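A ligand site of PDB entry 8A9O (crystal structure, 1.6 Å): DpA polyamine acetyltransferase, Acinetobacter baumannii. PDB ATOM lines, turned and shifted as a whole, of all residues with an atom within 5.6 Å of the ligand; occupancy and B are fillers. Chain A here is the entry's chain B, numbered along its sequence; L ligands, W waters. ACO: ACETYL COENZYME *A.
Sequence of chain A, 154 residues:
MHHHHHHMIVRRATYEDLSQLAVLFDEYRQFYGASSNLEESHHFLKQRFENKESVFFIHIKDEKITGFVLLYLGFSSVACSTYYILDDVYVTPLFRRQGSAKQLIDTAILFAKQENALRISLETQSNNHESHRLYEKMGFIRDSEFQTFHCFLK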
ATOM      1  N   TYR A  28      -3.811   0.644  30.274  1.00  0.00           N
ATOM      2  CA  TYR A  28      -3.604   0.520  28.837  1.00  0.00           C
ATOM      3  C   TYR A  28      -4.951   0.539  28.125  1.00  0.00           C
ATOM      4  O   TYR A  28      -5.110   1.248  27.144  1.00  0.00           O
ATOM      5  CB  TYR A  28      -2.842  -0.765  28.526  1.00  0.00           C
ATOM      6  CG  TYR A  28      -2.761  -1.121  27.056  1.00  0.00           C
ATOM      7  CD1 TYR A  28      -1.919  -0.409  26.195  1.00  0.00           C
ATOM      8  CD2 TYR A  28      -3.472  -2.195  26.532  1.00  0.00           C
ATOM      9  CE1 TYR A  28      -1.806  -0.756  24.856  1.00  0.00           C
ATOM     10  CE2 TYR A  28      -3.358  -2.543  25.194  1.00  0.00           C
ATOM     11  CZ  TYR A  28      -2.539  -1.815  24.351  1.00  0.00           C
ATOM     12  OH  TYR A  28      -2.432  -2.175  23.027  1.00  0.00           O
ATOM     13  N   PHE A  31      -6.310   4.042  27.910  1.00  0.00           N
ATOM     14  CA  PHE A  31      -5.649   4.860  26.890  1.00  0.00           C
ATOM     15  C   PHE A  31      -6.387   4.770  25.555  1.00  0.00           C
ATOM     16  O   PHE A  31      -6.474   5.753  24.818  1.00  0.00           O
ATOM     17  CB  PHE A  31      -4.165   4.450  26.722  1.00  0.00           C
ATOM     18  N   TYR A  32      -6.922   3.587  25.241  1.00  0.00           N
ATOM     19  CA  TYR A  32      -7.684   3.389  24.024  1.00  0.00           C
ATOM     20  C   TYR A  32      -9.190   3.626  24.169  1.00  0.00           C
ATOM     21  O   TYR A  32      -9.949   3.201  23.310  1.00  0.00           O
ATOM     22  CB  TYR A  32      -7.452   2.005  23.458  1.00  0.00           C
ATOM     23  CG  TYR A  32      -6.128   1.861  22.752  1.00  0.00           C
ATOM     24  CD1 TYR A  32      -5.963   2.294  21.445  1.00  0.00           C
ATOM     25  CD2 TYR A  32      -5.037   1.297  23.394  1.00  0.00           C
ATOM     26  CE1 TYR A  32      -4.753   2.151  20.778  1.00  0.00           C
ATOM     27  CE2 TYR A  32      -3.817   1.165  22.741  1.00  0.00           C
ATOM     28  CZ  TYR A  32      -3.676   1.597  21.437  1.00  0.00           C
ATOM     29  OH  TYR A  32      -2.473   1.475  20.786  1.00  0.00           O
ATOM     30  N   LEU A  86       3.482  -8.033  17.860  1.00  0.00           N
ATOM     31  CA  LEU A  86       3.592  -7.243  19.079  1.00  0.00           C
ATOM     32  C   LEU A  86       2.224  -6.556  19.205  1.00  0.00           C
ATOM     33  O   LEU A  86       1.910  -5.627  18.427  1.00  0.00           O
ATOM     34  CB  LEU A  86       4.727  -6.227  18.925  1.00  0.00           C
ATOM     35  CG  LEU A  86       5.034  -5.398  20.146  1.00  0.00           C
ATOM     36  CD1 LEU A  86       6.392  -4.773  20.039  1.00  0.00           C
ATOM     37  CD2 LEU A  86       4.088  -4.259  20.267  1.00  0.00           C
ATOM     38  N   ASP A  87       1.371  -7.100  20.058  1.00  0.00           N
ATOM     39  CA  ASP A  87      -0.031  -6.671  20.149  1.00  0.00           C
ATOM     40  C   ASP A  87      -0.245  -5.466  21.038  1.00  0.00           C
ATOM     41  O   ASP A  87      -1.034  -4.575  20.695  1.00  0.00           O
ATOM     42  CB  ASP A  87      -0.897  -7.846  20.660  1.00  0.00           C
ATOM     43  CG  ASP A  87      -2.341  -7.830  20.200  1.00  0.00           C
ATOM     44  OD1 ASP A  87      -2.678  -7.017  19.325  1.00  0.00           O
ATOM     45  OD2 ASP A  87      -3.126  -8.661  20.701  1.00  0.00           O
ATOM     46  N   ASP A  88       0.381  -5.460  22.212  1.00  0.00           N
ATOM     47  CA  ASP A  88       0.206  -4.380  23.172  1.00  0.00           C
ATOM     48  C   ASP A  88       1.578  -3.961  23.766  1.00  0.00           C
ATOM     49  O   ASP A  88       2.434  -4.816  24.015  1.00  0.00           O
ATOM     50  CB  ASP A  88      -0.654  -4.874  24.373  1.00  0.00           C
ATOM     51  CG  ASP A  88      -2.016  -5.509  24.122  1.00  0.00           C
ATOM     52  OD1 ASP A  88      -2.699  -5.097  23.157  1.00  0.00           O
ATOM     53  OD2 ASP A  88      -2.433  -6.376  24.944  1.00  0.00           O
ATOM     54  N   VAL A  89       1.786  -2.651  23.966  1.00  0.00           N
ATOM     55  CA  VAL A  89       3.021  -2.131  24.638  1.00  0.00           C
ATOM     56  C   VAL A  89       2.575  -0.935  25.497  1.00  0.00           C
ATOM     57  O   VAL A  89       1.866  -0.076  24.989  1.00  0.00           O
ATOM     58  CB  VAL A  89       4.148  -1.711  23.685  1.00  0.00           C
ATOM     59  CG1 VAL A  89       4.823  -2.899  23.036  1.00  0.00           C
ATOM     60  CG2 VAL A  89       3.675  -0.721  22.634  1.00  0.00           C
ATOM     61  N   TYR A  90       2.948  -0.936  26.773  1.00  0.00           N
ATOM     62  CA  TYR A  90       2.514   0.143  27.658  1.00  0.00           C
ATOM     63  C   TYR A  90       3.501   0.351  28.805  1.00  0.00           C
ATOM     64  O   TYR A  90       3.977  -0.623  29.383  1.00  0.00           O
ATOM     65  CB  TYR A  90       1.128  -0.227  28.245  1.00  0.00           C
ATOM     66  CG  TYR A  90       0.575   0.797  29.201  1.00  0.00           C
ATOM     67  CD1 TYR A  90      -0.024   1.957  28.726  1.00  0.00           C
ATOM     68  CD2 TYR A  90       0.728   0.656  30.574  1.00  0.00           C
ATOM     69  CE1 TYR A  90      -0.473   2.944  29.593  1.00  0.00           C
ATOM     70  CE2 TYR A  90       0.312   1.655  31.450  1.00  0.00           C
ATOM     71  CZ  TYR A  90      -0.298   2.788  30.946  1.00  0.00           C
ATOM     72  OH  TYR A  90      -0.755   3.770  31.792  1.00  0.00           O
ATOM     73  N   VAL A  91       3.771   1.608  29.136  1.00  0.00           N
ATOM     74  CA  VAL A  91       4.575   1.979  30.286  1.00  0.00           C
ATOM     75  C   VAL A  91       3.759   3.003  31.082  1.00  0.00           C
ATOM     76  O   VAL A  91       3.136   3.894  30.470  1.00  0.00           O
ATOM     77  CB  VAL A  91       5.958   2.544  29.884  1.00  0.00           C
ATOM     78  CG1 VAL A  91       6.715   3.084  31.096  1.00  0.00           C
ATOM     79  CG2 VAL A  91       6.796   1.492  29.169  1.00  0.00           C
ATOM     80  N   THR A  92       3.644   2.825  32.399  1.00  0.00           N
ATOM     81  CA  THR A  92       2.826   3.731  33.216  1.00  0.00           C
ATOM     82  C   THR A  92       3.466   5.131  33.206  1.00  0.00           C
ATOM     83  O   THR A  92       4.699   5.263  33.142  1.00  0.00           O
ATOM     84  CB  THR A  92       2.578   3.127  34.617  1.00  0.00           C
ATOM     85  OG1 THR A  92       1.532   3.841  35.298  1.00  0.00           O
ATOM     86  CG2 THR A  92       3.831   3.047  35.432  1.00  0.00           C
ATOM     87  N   PHE A  95       6.771   6.321  34.999  1.00  0.00           N
ATOM     88  CA  PHE A  95       8.020   5.702  34.595  1.00  0.00           C
ATOM     89  C   PHE A  95       8.413   5.903  33.129  1.00  0.00           C
ATOM     90  O   PHE A  95       9.374   5.287  32.669  1.00  0.00           O
ATOM     91  CB  PHE A  95       7.995   4.195  34.934  1.00  0.00           C
ATOM     92  CG  PHE A  95       7.969   3.956  36.412  1.00  0.00           C
ATOM     93  CD1 PHE A  95       9.124   4.057  37.168  1.00  0.00           C
ATOM     94  CD2 PHE A  95       6.793   3.661  37.066  1.00  0.00           C
ATOM     95  CE1 PHE A  95       9.092   3.877  38.544  1.00  0.00           C
ATOM     96  CE2 PHE A  95       6.762   3.464  38.441  1.00  0.00           C
ATOM     97  CZ  PHE A  95       7.912   3.584  39.170  1.00  0.00           C
ATOM     98  N   ARG A  96       7.761   6.829  32.438  1.00  0.00           N
ATOM     99  CA  ARG A  96       8.068   7.063  31.038  1.00  0.00           C
ATOM    100  C   ARG A  96       9.362   7.829  30.807  1.00  0.00           C
ATOM    101  O   ARG A  96       9.848   8.553  31.685  1.00  0.00           O
ATOM    102  CB  ARG A  96       6.891   7.724  30.309  1.00  0.00           C
ATOM    103  CG  ARG A  96       5.744   6.755  30.123  1.00  0.00           C
ATOM    104  CD  ARG A  96       4.563   7.412  29.444  1.00  0.00           C
ATOM    105  NE  ARG A  96       3.436   6.486  29.460  1.00  0.00           N
ATOM    106  CZ  ARG A  96       2.202   6.773  29.087  1.00  0.00           C
ATOM    107  NH1 ARG A  96       1.898   7.985  28.634  1.00  0.00           N
ATOM    108  NH2 ARG A  96       1.247   5.854  29.148  1.00  0.00           N
ATOM    109  N   ARG A  97       9.916   7.627  29.605  1.00  0.00           N
ATOM    110  CA  ARG A  97      11.124   8.253  29.105  1.00  0.00           C
ATOM    111  C   ARG A  97      12.362   7.877  29.917  1.00  0.00           C
ATOM    112  O   ARG A  97      13.279   8.685  30.104  1.00  0.00           O
ATOM    113  CB  ARG A  97      10.946   9.782  28.956  1.00  0.00           C
ATOM    114  CG  ARG A  97      11.555  10.312  27.659  1.00  0.00           C
ATOM    115  CD  ARG A  97      10.948   9.739  26.394  1.00  0.00           C
ATOM    116  NE  ARG A  97      11.767  10.092  25.218  1.00  0.00           N
ATOM    117  CZ  ARG A  97      11.554  11.166  24.456  1.00  0.00           C
ATOM    118  NH1 ARG A  97      12.345  11.415  23.428  1.00  0.00           N
ATOM    119  NH2 ARG A  97      10.534  11.975  24.702  1.00  0.00           N
ATOM    120  N   GLN A  98      12.390   6.611  30.393  1.00  0.00           N
ATOM    121  CA  GLN A  98      13.522   6.040  31.142  1.00  0.00           C
ATOM    122  C   GLN A  98      14.063   4.770  30.465  1.00  0.00           C
ATOM    123  O   GLN A  98      14.863   4.067  31.091  1.00  0.00           O
ATOM    124  CB  GLN A  98      13.064   5.634  32.539  1.00  0.00           C
ATOM    125  CG  GLN A  98      12.789   6.787  33.484  1.00  0.00           C
ATOM    126  CD  GLN A  98      12.355   6.297  34.857  1.00  0.00           C
ATOM    127  OE1 GLN A  98      12.504   5.116  35.220  1.00  0.00           O
ATOM    128  NE2 GLN A  98      11.777   7.188  35.643  1.00  0.00           N
ATOM    129  N   GLY A  99      13.546   4.412  29.301  1.00  0.00           N
ATOM    130  CA  GLY A  99      13.993   3.228  28.593  1.00  0.00           C
ATOM    131  C   GLY A  99      13.222   1.958  28.861  1.00  0.00           C
ATOM    132  O   GLY A  99      13.603   0.917  28.324  1.00  0.00           O
ATOM    133  N   SER A 100      12.122   1.990  29.654  1.00  0.00           N
ATOM    134  CA  SER A 100      11.332   0.773  29.893  1.00  0.00           C
ATOM    135  C   SER A 100      10.843   0.120  28.575  1.00  0.00           C
ATOM    136  O   SER A 100      11.029  -1.077  28.380  1.00  0.00           O
ATOM    137  CB  SER A 100      10.111   1.016  30.783  1.00  0.00           C
ATOM    138  OG  SER A 100      10.462   1.270  32.138  1.00  0.00           O
ATOM    139  N   ALA A 101      10.200   0.915  27.688  1.00  0.00           N
ATOM    140  CA  ALA A 101       9.675   0.356  26.425  1.00  0.00           C
ATOM    141  C   ALA A 101      10.808  -0.150  25.544  1.00  0.00           C
ATOM    142  O   ALA A 101      10.704  -1.236  24.985  1.00  0.00           O
ATOM    143  CB  ALA A 101       8.843   1.390  25.690  1.00  0.00           C
ATOM    144  N   LYS A 102      11.918   0.581  25.490  1.00  0.00           N
ATOM    145  CA  LYS A 102      13.090   0.154  24.723  1.00  0.00           C
ATOM    146  C   LYS A 102      13.582  -1.221  25.258  1.00  0.00           C
ATOM    147  O   LYS A 102      13.781  -2.150  24.469  1.00  0.00           O
ATOM    148  CB  LYS A 102      14.232   1.202  24.864  1.00  0.00           C
ATOM    149  CG  LYS A 102      15.531   0.729  24.219  1.00  0.00           C
ATOM    150  CD  LYS A 102      16.655   1.739  24.403  1.00  0.00           C
ATOM    151  CE  LYS A 102      17.923   0.999  24.805  1.00  0.00           C
ATOM    152  NZ  LYS A 102      18.265  -0.106  23.861  1.00  0.00           N
ATOM    153  N   GLN A 103      13.720  -1.354  26.590  1.00  0.00           N
ATOM    154  CA  GLN A 103      14.182  -2.624  27.179  1.00  0.00           C
ATOM    155  C   GLN A 103      13.183  -3.760  26.946  1.00  0.00           C
ATOM    156  O   GLN A 103      13.585  -4.900  26.664  1.00  0.00           O
ATOM    157  CB  GLN A 103      14.486  -2.445  28.671  1.00  0.00           C
ATOM    158  CG  GLN A 103      15.670  -1.500  28.878  1.00  0.00           C
ATOM    159  CD  GLN A 103      15.770  -1.002  30.294  1.00  0.00           C
ATOM    160  OE1 GLN A 103      15.382  -1.681  31.239  1.00  0.00           O
ATOM    161  NE2 GLN A 103      16.273   0.197  30.457  1.00  0.00           N
ATOM    162  N   LEU A 122       3.614  -5.398  13.753  1.00  0.00           N
ATOM    163  CA  LEU A 122       2.621  -4.723  14.588  1.00  0.00           C
ATOM    164  C   LEU A 122       1.849  -3.697  13.757  1.00  0.00           C
ATOM    165  O   LEU A 122       2.275  -3.336  12.655  1.00  0.00           O
ATOM    166  CB  LEU A 122       3.336  -4.020  15.774  1.00  0.00           C
ATOM    167  CG  LEU A 122       4.343  -2.924  15.444  1.00  0.00           C
ATOM    168  CD1 LEU A 122       3.669  -1.545  15.203  1.00  0.00           C
ATOM    169  CD2 LEU A 122       5.333  -2.771  16.544  1.00  0.00           C
ATOM    170  N   GLU A 123       0.756  -3.202  14.322  1.00  0.00           N
ATOM    171  CA  GLU A 123      -0.033  -2.098  13.750  1.00  0.00           C
ATOM    172  C   GLU A 123      -0.217  -1.075  14.851  1.00  0.00           C
ATOM    173  O   GLU A 123      -0.585  -1.431  15.980  1.00  0.00           O
ATOM    174  CB  GLU A 123      -1.419  -2.596  13.289  1.00  0.00           C
ATOM    175  N   THR A 124       0.007   0.209  14.546  1.00  0.00           N
ATOM    176  CA  THR A 124      -0.187   1.268  15.536  1.00  0.00           C
ATOM    177  C   THR A 124      -0.959   2.392  14.862  1.00  0.00           C
ATOM    178  O   THR A 124      -0.919   2.504  13.638  1.00  0.00           O
ATOM    179  CB  THR A 124       1.184   1.729  16.111  1.00  0.00           C
ATOM    180  OG1 THR A 124       0.966   2.613  17.201  1.00  0.00           O
ATOM    181  CG2 THR A 124       2.079   2.385  15.095  1.00  0.00           C
ATOM    182  N   ASN A 128      -0.139   8.184  16.162  1.00  0.00           N
ATOM    183  CA  ASN A 128       0.570   7.926  17.413  1.00  0.00           C
ATOM    184  C   ASN A 128       2.056   8.243  17.208  1.00  0.00           C
ATOM    185  O   ASN A 128       2.861   7.347  16.968  1.00  0.00           O
ATOM    186  CB  ASN A 128       0.360   6.477  17.856  1.00  0.00           C
ATOM    187  CG  ASN A 128       0.832   6.203  19.263  1.00  0.00           C
ATOM    188  OD1 ASN A 128       1.735   6.887  19.796  1.00  0.00           O
ATOM    189  ND2 ASN A 128       0.260   5.194  19.899  1.00  0.00           N
ATOM    190  N   HIS A 129       2.414   9.538  17.356  1.00  0.00           N
ATOM    191  CA  HIS A 129       3.781  10.036  17.168  1.00  0.00           C
ATOM    192  C   HIS A 129       4.770   9.274  18.027  1.00  0.00           C
ATOM    193  O   HIS A 129       5.809   8.843  17.524  1.00  0.00           O
ATOM    194  CB  HIS A 129       3.860  11.546  17.523  1.00  0.00           C
ATOM    195  CG  HIS A 129       5.264  12.079  17.589  1.00  0.00           C
ATOM    196  ND1 HIS A 129       6.013  12.301  16.437  1.00  0.00           N
ATOM    197  CD2 HIS A 129       6.026  12.408  18.671  1.00  0.00           C
ATOM    198  CE1 HIS A 129       7.202  12.716  16.858  1.00  0.00           C
ATOM    199  NE2 HIS A 129       7.250  12.813  18.190  1.00  0.00           N
ATOM    200  N   GLU A 130       4.461   9.123  19.318  1.00  0.00           N
ATOM    201  CA  GLU A 130       5.351   8.507  20.295  1.00  0.00           C
ATOM    202  C   GLU A 130       5.686   7.077  19.910  1.00  0.00           C
ATOM    203  O   GLU A 130       6.862   6.699  19.928  1.00  0.00           O
ATOM    204  CB  GLU A 130       4.704   8.548  21.693  1.00  0.00           C
ATOM    205  CG  GLU A 130       4.479   9.952  22.224  1.00  0.00           C
ATOM    206  CD  GLU A 130       3.312  10.730  21.645  1.00  0.00           C
ATOM    207  OE1 GLU A 130       2.414  10.116  21.023  1.00  0.00           O
ATOM    208  OE2 GLU A 130       3.305  11.978  21.831  1.00  0.00           O
ATOM    209  N   SER A 131       4.669   6.280  19.552  1.00  0.00           N
ATOM    210  CA  SER A 131       4.927   4.893  19.190  1.00  0.00           C
ATOM    211  C   SER A 131       5.755   4.796  17.910  1.00  0.00           C
ATOM    212  O   SER A 131       6.647   3.958  17.854  1.00  0.00           O
ATOM    213  CB  SER A 131       3.629   4.094  19.082  1.00  0.00           C
ATOM    214  OG  SER A 131       2.939   4.383  17.880  1.00  0.00           O
ATOM    215  N   ARG A 133       8.066   6.811  16.820  1.00  0.00           N
ATOM    216  CA  ARG A 133       9.448   7.121  17.155  1.00  0.00           C
ATOM    217  C   ARG A 133      10.097   5.954  17.909  1.00  0.00           C
ATOM    218  O   ARG A 133      11.247   5.608  17.624  1.00  0.00           O
ATOM    219  CB  ARG A 133       9.530   8.415  17.947  1.00  0.00           C
ATOM    220  CG  ARG A 133       8.846   9.607  17.243  1.00  0.00           C
ATOM    221  CD  ARG A 133       9.574  10.119  15.991  1.00  0.00           C
ATOM    222  NE  ARG A 133       9.320   9.356  14.752  1.00  0.00           N
ATOM    223  CZ  ARG A 133       8.192   9.426  14.047  1.00  0.00           C
ATOM    224  NH1 ARG A 133       7.161  10.122  14.494  1.00  0.00           N
ATOM    225  NH2 ARG A 133       8.087   8.746  12.913  1.00  0.00           N
ATOM    226  N   LEU A 134       9.350   5.332  18.819  1.00  0.00           N
ATOM    227  CA  LEU A 134       9.820   4.156  19.564  1.00  0.00           C
ATOM    228  C   LEU A 134      10.176   3.024  18.587  1.00  0.00           C
ATOM    229  O   LEU A 134      11.295   2.497  18.632  1.00  0.00           O
ATOM    230  CB  LEU A 134       8.708   3.711  20.556  1.00  0.00           C
ATOM    231  CG  LEU A 134       8.882   2.337  21.203  1.00  0.00           C
ATOM    232  CD1 LEU A 134      10.092   2.313  22.107  1.00  0.00           C
ATOM    233  CD2 LEU A 134       7.620   1.933  21.977  1.00  0.00           C
ATOM    234  N   TYR A 135       9.248   2.659  17.714  1.00  0.00           N
ATOM    235  CA  TYR A 135       9.459   1.523  16.817  1.00  0.00           C
ATOM    236  C   TYR A 135      10.603   1.770  15.856  1.00  0.00           C
ATOM    237  O   TYR A 135      11.450   0.882  15.681  1.00  0.00           O
ATOM    238  CB  TYR A 135       8.156   1.132  16.107  1.00  0.00           C
ATOM    239  CG  TYR A 135       7.067   0.764  17.079  1.00  0.00           C
ATOM    240  CD1 TYR A 135       7.331  -0.010  18.198  1.00  0.00           C
ATOM    241  CD2 TYR A 135       5.754   1.149  16.846  1.00  0.00           C
ATOM    242  CE1 TYR A 135       6.330  -0.353  19.101  1.00  0.00           C
ATOM    243  CE2 TYR A 135       4.740   0.806  17.744  1.00  0.00           C
ATOM    244  CZ  TYR A 135       5.029   0.050  18.860  1.00  0.00           C
ATOM    245  OH  TYR A 135       4.026  -0.285  19.728  1.00  0.00           O
ATOM    246  N   LYS A 137      13.184   3.661  16.423  1.00  0.00           N
ATOM    247  CA  LYS A 137      14.424   3.554  17.209  1.00  0.00           C
ATOM    248  C   LYS A 137      14.845   2.094  17.362  1.00  0.00           C
ATOM    249  O   LYS A 137      16.034   1.773  17.310  1.00  0.00           O
ATOM    250  CB  LYS A 137      14.215   4.179  18.603  1.00  0.00           C
ATOM    251  CG  LYS A 137      15.515   4.262  19.414  1.00  0.00           C
ATOM    252  CD  LYS A 137      15.241   4.626  20.871  1.00  0.00           C
ATOM    253  CE  LYS A 137      16.507   4.891  21.635  1.00  0.00           C
ATOM    254  NZ  LYS A 137      17.004   6.286  21.411  1.00  0.00           N
HETATM  255  N1A ACO L   1       7.792  11.488  22.333  1.00  0.00           N
HETATM  256  C2A ACO L   1       8.596  11.086  21.345  1.00  0.00           C
HETATM  257  N3A ACO L   1       9.272   9.940  21.236  1.00  0.00           N
HETATM  258  C4A ACO L   1       9.091   9.170  22.308  1.00  0.00           C
HETATM  259  C5A ACO L   1       8.288   9.449  23.410  1.00  0.00           C
HETATM  260  C6A ACO L   1       7.610  10.677  23.410  1.00  0.00           C
HETATM  261  N6A ACO L   1       6.832  11.097  24.410  1.00  0.00           N
HETATM  262  N7A ACO L   1       8.329   8.400  24.322  1.00  0.00           N
HETATM  263  C8A ACO L   1       9.148   7.544  23.774  1.00  0.00           C
HETATM  264  N9A ACO L   1       9.647   7.938  22.563  1.00  0.00           N
HETATM  265  C1B ACO L   1      10.534   7.188  21.689  1.00  0.00           C
HETATM  266  C2B ACO L   1      11.915   7.822  21.544  1.00  0.00           C
HETATM  267  O2B ACO L   1      12.466   7.450  20.287  1.00  0.00           O
HETATM  268  C3B ACO L   1      12.620   7.131  22.701  1.00  0.00           C
HETATM  269  O3B ACO L   1      14.056   7.232  22.662  1.00  0.00           O
HETATM  270  P3B ACO L   1      14.767   8.450  23.439  1.00  0.00           P
HETATM  271  O7A ACO L   1      14.229   8.656  24.832  1.00  0.00           O
HETATM  272  O8A ACO L   1      14.523   9.676  22.563  1.00  0.00           O
HETATM  273  O9A ACO L   1      16.262   8.122  23.419  1.00  0.00           O
HETATM  274  C4B ACO L   1      12.149   5.707  22.533  1.00  0.00           C
HETATM  275  O4B ACO L   1      10.730   5.890  22.259  1.00  0.00           O
HETATM  276  C5B ACO L   1      12.338   4.877  23.767  1.00  0.00           C
HETATM  277  O5B ACO L   1      11.637   5.494  24.862  1.00  0.00           O
HETATM  278  P1A ACO L   1      11.277   4.760  26.257  1.00  0.00           P
HETATM  279  O1A ACO L   1      11.735   5.655  27.345  1.00  0.00           O
HETATM  280  O2A ACO L   1      11.782   3.357  26.215  1.00  0.00           O
HETATM  281  O3A ACO L   1       9.699   4.756  26.117  1.00  0.00           O
HETATM  282  P2A ACO L   1       8.683   4.662  27.334  1.00  0.00           P
HETATM  283  O4A ACO L   1       9.169   3.677  28.311  1.00  0.00           O
HETATM  284  O5A ACO L   1       8.332   6.037  27.817  1.00  0.00           O
HETATM  285  O6A ACO L   1       7.338   4.053  26.651  1.00  0.00           O
HETATM  286  CBP ACO L   1       5.408   4.238  25.201  1.00  0.00           C
HETATM  287  CCP ACO L   1       6.892   4.561  25.391  1.00  0.00           C
HETATM  288  CDP ACO L   1       5.003   4.637  23.777  1.00  0.00           C
HETATM  289  CEP ACO L   1       5.216   2.726  25.386  1.00  0.00           C
HETATM  290  CAP ACO L   1       4.565   5.017  26.257  1.00  0.00           C
HETATM  291  OAP ACO L   1       4.627   6.418  26.034  1.00  0.00           O
HETATM  292  C9P ACO L   1       3.118   4.561  26.396  1.00  0.00           C
HETATM  293  O9P ACO L   1       2.851   3.617  27.125  1.00  0.00           O
HETATM  294  N8P ACO L   1       2.199   5.238  25.685  1.00  0.00           N
HETATM  295  C7P ACO L   1       0.795   4.850  25.622  1.00  0.00           C
HETATM  296  C6P ACO L   1       0.610   3.452  25.032  1.00  0.00           C
HETATM  297  C5P ACO L   1       1.043   3.381  23.578  1.00  0.00           C
HETATM  298  O5P ACO L   1       1.017   4.375  22.861  1.00  0.00           O
HETATM  299  N4P ACO L   1       1.453   2.189  23.141  1.00  0.00           N
HETATM  300  C3P ACO L   1       1.497   1.875  21.708  1.00  0.00           C
HETATM  301  C2P ACO L   1       0.805   0.590  21.310  1.00  0.00           C
HETATM  302  S1P ACO L   1       1.106   0.273  19.530  1.00  0.00           S
HETATM  303  C   ACO L   1       1.147  -1.503  19.446  1.00  0.00           C
HETATM  304  O   ACO L   1       0.833  -2.207  20.356  1.00  0.00           O
HETATM  305  CH3 ACO L   1       1.632  -2.011  18.126  1.00  0.00           C
HETATM  306  O   HOH W   1       6.590  13.891  22.500  1.00  0.00           O
HETATM  307  O   HOH W   2      15.190  10.652  26.219  1.00  0.00           O
HETATM  308  O   HOH W   3       4.894  13.576  24.478  1.00  0.00           O
HETATM  309  O   HOH W   4      14.113   6.878  26.736  1.00  0.00           O
HETATM  310  O   HOH W   5      10.536   4.411  30.411  1.00  0.00           O
HETATM  311  O   HOH W   6       1.521   7.139  22.921  1.00  0.00           O
HETATM  312  O   HOH W   7       6.898   7.835  26.573  1.00  0.00           O
HETATM  313  O   HOH W   8       6.477  10.294  27.420  1.00  0.00           O
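The backbone carbonyl oxygen (O) of Val 91 lies within hydrogen-bond range of the guanidinium group (NE) of Arg 96 (2.8 Å). The side-chain carboxylate (OD1) of Asp 88 is in hydrogen-bond range of the side-chain hydroxyl (OH) of Tyr 28 (2.9 Å). ND1 of His 129 is in hydrogen-bond range of NH1 of Arg 133, at 3.1 Å. O of Gly 99 lies close to NE2 of Gln 103 (3.5 Å). The side-chain amide oxygen (OD1) of Asn 128 is in hydrogen-bond range of the backbone NH (N) of Ser 131. OG1 of Thr 124 lies within hydrogen-bond range of OG of Ser 131 (2.7 Å).
Water W6 bridges O5P of the ligand (2.8 Å) and OD1 of Asn 128 (3.1 Å). Water W3 lies within hydrogen-bond range of a nitrogen (N6A) of the ligand and the side-chain carboxylate of Glu 130.
O of the ligand sits close to O of Asp 87 (3.0 Å). OH of Tyr 32 touches C2P of the ligand, 3.4 Å away. O of Leu 86 touches CH3 of the ligand, at 3.6 Å. Asp 88 touches the ligand (CA to O, 3.6 Å). Tyr 90 touches the ligand. N of Ser 100 touches O4A of the ligand, 3.7 Å away. CB of Leu 122 touches CH3 of the ligand, 3.5 Å away. O of Glu 123 touches CH3 of the ligand, 3.1 Å away. His 129 touches the ligand (NE2 to C2A, 3.8 Å). Glu 130 touches the ligand (CG to N6A, 3.4 Å). Leu 134 touches the ligand. Hydrophobic or aromatic side chains within 4 Å of the ligand: Leu 86, Val 89, Tyr 90, Val 91, Ala 101, Leu 122, His 129, Leu 134 and Tyr 135. Along chain A the residues within 4 Å of the ligand span positions 32 to 137.
A sulfur (S1P) of the ligand lies close to the side-chain hydroxyl (OG1) of Thr 124, at 3.3 Å. The guanidinium group of Arg 97 lies within salt-bridge range of an oxygen (O7A) of the ligand, at 2.9 Å. The backbone NH (N) of Gly 99 is in hydrogen-bond range of an oxygen (O1A) of the ligand (2.9 Å). The side-chain amino group (NZ) of Lys 137 is in salt-bridge range of an oxygen (O9A) of the ligand (2.8 Å). S1P of the ligand lies close to OH of Tyr 135. O of Val 89 lies within hydrogen-bond range of N4P of the ligand (3.0 Å). The backbone NH of Val 91 sits at hydrogen-bond distance from an oxygen (O9P) of the ligand (3.0 Å). The guanidinium group (NH2) of Arg 96 is in hydrogen-bond range of an oxygen (O9P) of the ligand (3.4 Å). An oxygen (O5P) of the ligand is in hydrogen-bond range of the side-chain amide nitrogen (ND2) of Asn 128 (3.2 Å). An oxygen (O5A) of the ligand sits at hydrogen-bond distance from the backbone NH of Arg 97, at 2.9 Å. The backbone carbonyl oxygen of Arg 133 is in hydrogen-bond range of an oxygen (O2B) of the ligand, at 3.5 Å. N of Ala 101 is in hydrogen-bond range of O4A of the ligand. An oxygen (O1A) of the ligand lies within hydrogen-bond range of the backbone NH (N) of Gln 98, at 3.3 Å. The backbone NH of Lys 102 is in hydrogen-bond range of an oxygen (O2A) of the ligand.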
